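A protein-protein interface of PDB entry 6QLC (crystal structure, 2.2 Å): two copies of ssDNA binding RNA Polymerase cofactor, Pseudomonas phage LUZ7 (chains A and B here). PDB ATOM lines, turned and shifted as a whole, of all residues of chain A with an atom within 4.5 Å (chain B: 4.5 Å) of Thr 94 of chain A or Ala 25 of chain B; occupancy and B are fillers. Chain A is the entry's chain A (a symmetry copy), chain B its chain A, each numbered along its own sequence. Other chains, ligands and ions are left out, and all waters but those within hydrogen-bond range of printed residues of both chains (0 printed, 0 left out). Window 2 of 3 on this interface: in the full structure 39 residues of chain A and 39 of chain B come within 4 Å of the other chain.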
ATOM      1  N   GLY A  92      -8.047  -4.358   7.658  1.00  0.00           N
ATOM      2  CA  GLY A  92      -8.442  -4.043   9.023  1.00  0.00           C
ATOM      3  C   GLY A  92      -8.045  -5.129  10.001  1.00  0.00           C
ATOM      4  O   GLY A  92      -8.208  -6.315   9.723  1.00  0.00           O
ATOM      5  N   VAL A  93      -7.522  -4.705  11.154  1.00  0.00           N
ATOM      6  CA  VAL A  93      -7.152  -5.603  12.248  1.00  0.00           C
ATOM      7  C   VAL A  93      -8.170  -5.455  13.374  1.00  0.00           C
ATOM      8  O   VAL A  93      -8.457  -4.337  13.827  1.00  0.00           O
ATOM      9  CB  VAL A  93      -5.723  -5.329  12.754  1.00  0.00           C
ATOM     10  CG1 VAL A  93      -5.530  -3.860  13.104  1.00  0.00           C
ATOM     11  CG2 VAL A  93      -5.407  -6.206  13.953  1.00  0.00           C
ATOM     12  N   THR A  94      -8.727  -6.579  13.816  1.00  0.00           N
ATOM     13  CA  THR A  94      -9.661  -6.558  14.931  1.00  0.00           C
ATOM     14  C   THR A  94      -8.903  -6.526  16.254  1.00  0.00           C
ATOM     15  O   THR A  94      -7.705  -6.814  16.328  1.00  0.00           O
ATOM     16  CB  THR A  94     -10.587  -7.777  14.910  1.00  0.00           C
ATOM     17  OG1 THR A  94      -9.817  -8.964  15.147  1.00  0.00           O
ATOM     18  CG2 THR A  94     -11.298  -7.891  13.572  1.00  0.00           C
ATOM     19  N   ARG A  95      -9.626  -6.171  17.309  1.00  0.00           N
ATOM     20  CA  ARG A  95      -9.040  -6.084  18.633  1.00  0.00           C
ATOM     21  C   ARG A  95      -8.823  -7.470  19.208  1.00  0.00           C
ATOM     22  O   ARG A  95      -9.618  -8.385  18.984  1.00  0.00           O
ATOM     23  CB  ARG A  95      -9.946  -5.297  19.572  1.00  0.00           C
ATOM     24  CG  ARG A  95     -10.156  -3.862  19.197  1.00  0.00           C
ATOM     25  CD  ARG A  95     -10.635  -3.096  20.417  1.00  0.00           C
ATOM     26  NE  ARG A  95     -12.089  -3.122  20.543  1.00  0.00           N
ATOM     27  CZ  ARG A  95     -12.766  -2.446  21.466  1.00  0.00           C
ATOM     28  NH1 ARG A  95     -12.119  -1.703  22.362  1.00  0.00           N
ATOM     29  NH2 ARG A  95     -14.090  -2.516  21.493  1.00  0.00           N
ATOM     30  N   SER A  96      -7.741  -7.617  19.957  1.00  0.00           N
ATOM     31  CA  SER A  96      -7.552  -8.820  20.743  1.00  0.00           C
ATOM     32  C   SER A  96      -8.552  -8.847  21.890  1.00  0.00           C
ATOM     33  O   SER A  96      -9.126  -7.820  22.279  1.00  0.00           O
ATOM     34  CB  SER A  96      -6.139  -8.877  21.309  1.00  0.00           C
ATOM     35  OG  SER A  96      -5.902  -7.758  22.147  1.00  0.00           O
ATOM     36  N   GLY B  24      -7.163 -13.389  21.250  1.00  0.00           N
ATOM     37  CA  GLY B  24      -6.256 -12.859  20.251  1.00  0.00           C
ATOM     38  C   GLY B  24      -6.977 -12.150  19.114  1.00  0.00           C
ATOM     39  O   GLY B  24      -8.209 -12.145  19.009  1.00  0.00           O
ATOM     40  N   ALA B  25      -6.174 -11.542  18.240  1.00  0.00           N
ATOM     41  CA  ALA B  25      -6.659 -10.717  17.141  1.00  0.00           C
ATOM     42  C   ALA B  25      -6.327 -11.357  15.796  1.00  0.00           C
ATOM     43  O   ALA B  25      -5.635 -12.376  15.719  1.00  0.00           O
ATOM     44  CB  ALA B  25      -6.064  -9.304  17.221  1.00  0.00           C
ATOM     45  N   SER B  26      -6.842 -10.741  14.727  1.00  0.00           N
ATOM     46  CA  SER B  26      -6.595 -11.198  13.361  1.00  0.00           C
ATOM     47  C   SER B  26      -6.810 -10.038  12.397  1.00  0.00           C
ATOM     48  O   SER B  26      -7.416  -9.021  12.746  1.00  0.00           O
ATOM     49  CB  SER B  26      -7.497 -12.380  12.979  1.00  0.00           C
ATOM     50  OG  SER B  26      -8.843 -12.147  13.352  1.00  0.00           O
ATOM     51  N   TYR B  28      -8.233  -8.557   8.614  1.00  0.00           N
ATOM     52  CA  TYR B  28      -9.357  -8.721   7.701  1.00  0.00           C
ATOM     53  C   TYR B  28      -9.112  -7.904   6.443  1.00  0.00           C
ATOM     54  O   TYR B  28      -8.529  -6.818   6.489  1.00  0.00           O
ATOM     55  CB  TYR B  28     -10.701  -8.282   8.352  1.00  0.00           C
ATOM     56  CG  TYR B  28     -11.244  -9.312   9.325  1.00  0.00           C
ATOM     57  CD1 TYR B  28     -10.518  -9.670  10.461  1.00  0.00           C
ATOM     58  CD2 TYR B  28     -12.459  -9.958   9.098  1.00  0.00           C
ATOM     59  CE1 TYR B  28     -10.979 -10.632  11.349  1.00  0.00           C
ATOM     60  CE2 TYR B  28     -12.938 -10.928   9.996  1.00  0.00           C
ATOM     61  CZ  TYR B  28     -12.186 -11.254  11.120  1.00  0.00           C
ATOM     62  OH  TYR B  28     -12.622 -12.202  12.024  1.00  0.00           O
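The backbone NH (N) of Thr 94 of chain A sits at hydrogen-bond distance from the backbone carbonyl oxygen (O) of Ser 26 of chain B (3.0 Å). The backbone carbonyl oxygen of Gly 92 of chain A lies within hydrogen-bond range of the backbone NH of Tyr 28 of chain B, 2.5 Å away.
Among the printed residues, merely in contact across the chains: Thr 94 of chain A with Ala 25 of chain B, Val 93 of chain A with Ser 26 of chain B, Thr 94 of chain A with Tyr 28 of chain B, Ser 96 of chain A with Ala 25 of chain B, Ser 96 of chain A with Gly 24 of chain B and Arg 95 of chain A with Ala 25 of chain B.
Of chain B, only Ala 25, Ser 26 and Tyr 28 come within 4 Å of Thr 94 of chain A. Of the printed residues of chain B, Ser 96 of chain A touches Gly 24 and Ala 25. Of the printed residues of chain A, Gly 24 of chain B touches Ser 96 (3.8 Å). Ala 25 of chain B touches just these residues of chain A: Thr 94 (3.1 Å), Arg 95 (3.9 Å) and Ser 96 (3.6 Å). The nearest printed residue of chain A that does not touch Ala 25 of chain B is Val 93 of chain A (4.6 Å).
Printed residues of chain A that touch a printed residue of chain B: Gly 92, Val 93, Thr 94, Arg 95 and Ser 96. Among the printed residues, 8 pairs touch across the chains. Among the printed residues, no Asp or Glu carboxylate lies within 4 Å of a Lys or Arg side-chain nitrogen of the other chain.
No position is printed for both chains. Of the 8 pairs that touch across the chains among the printed residues, none has its exchanged pair printed and touching as well.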
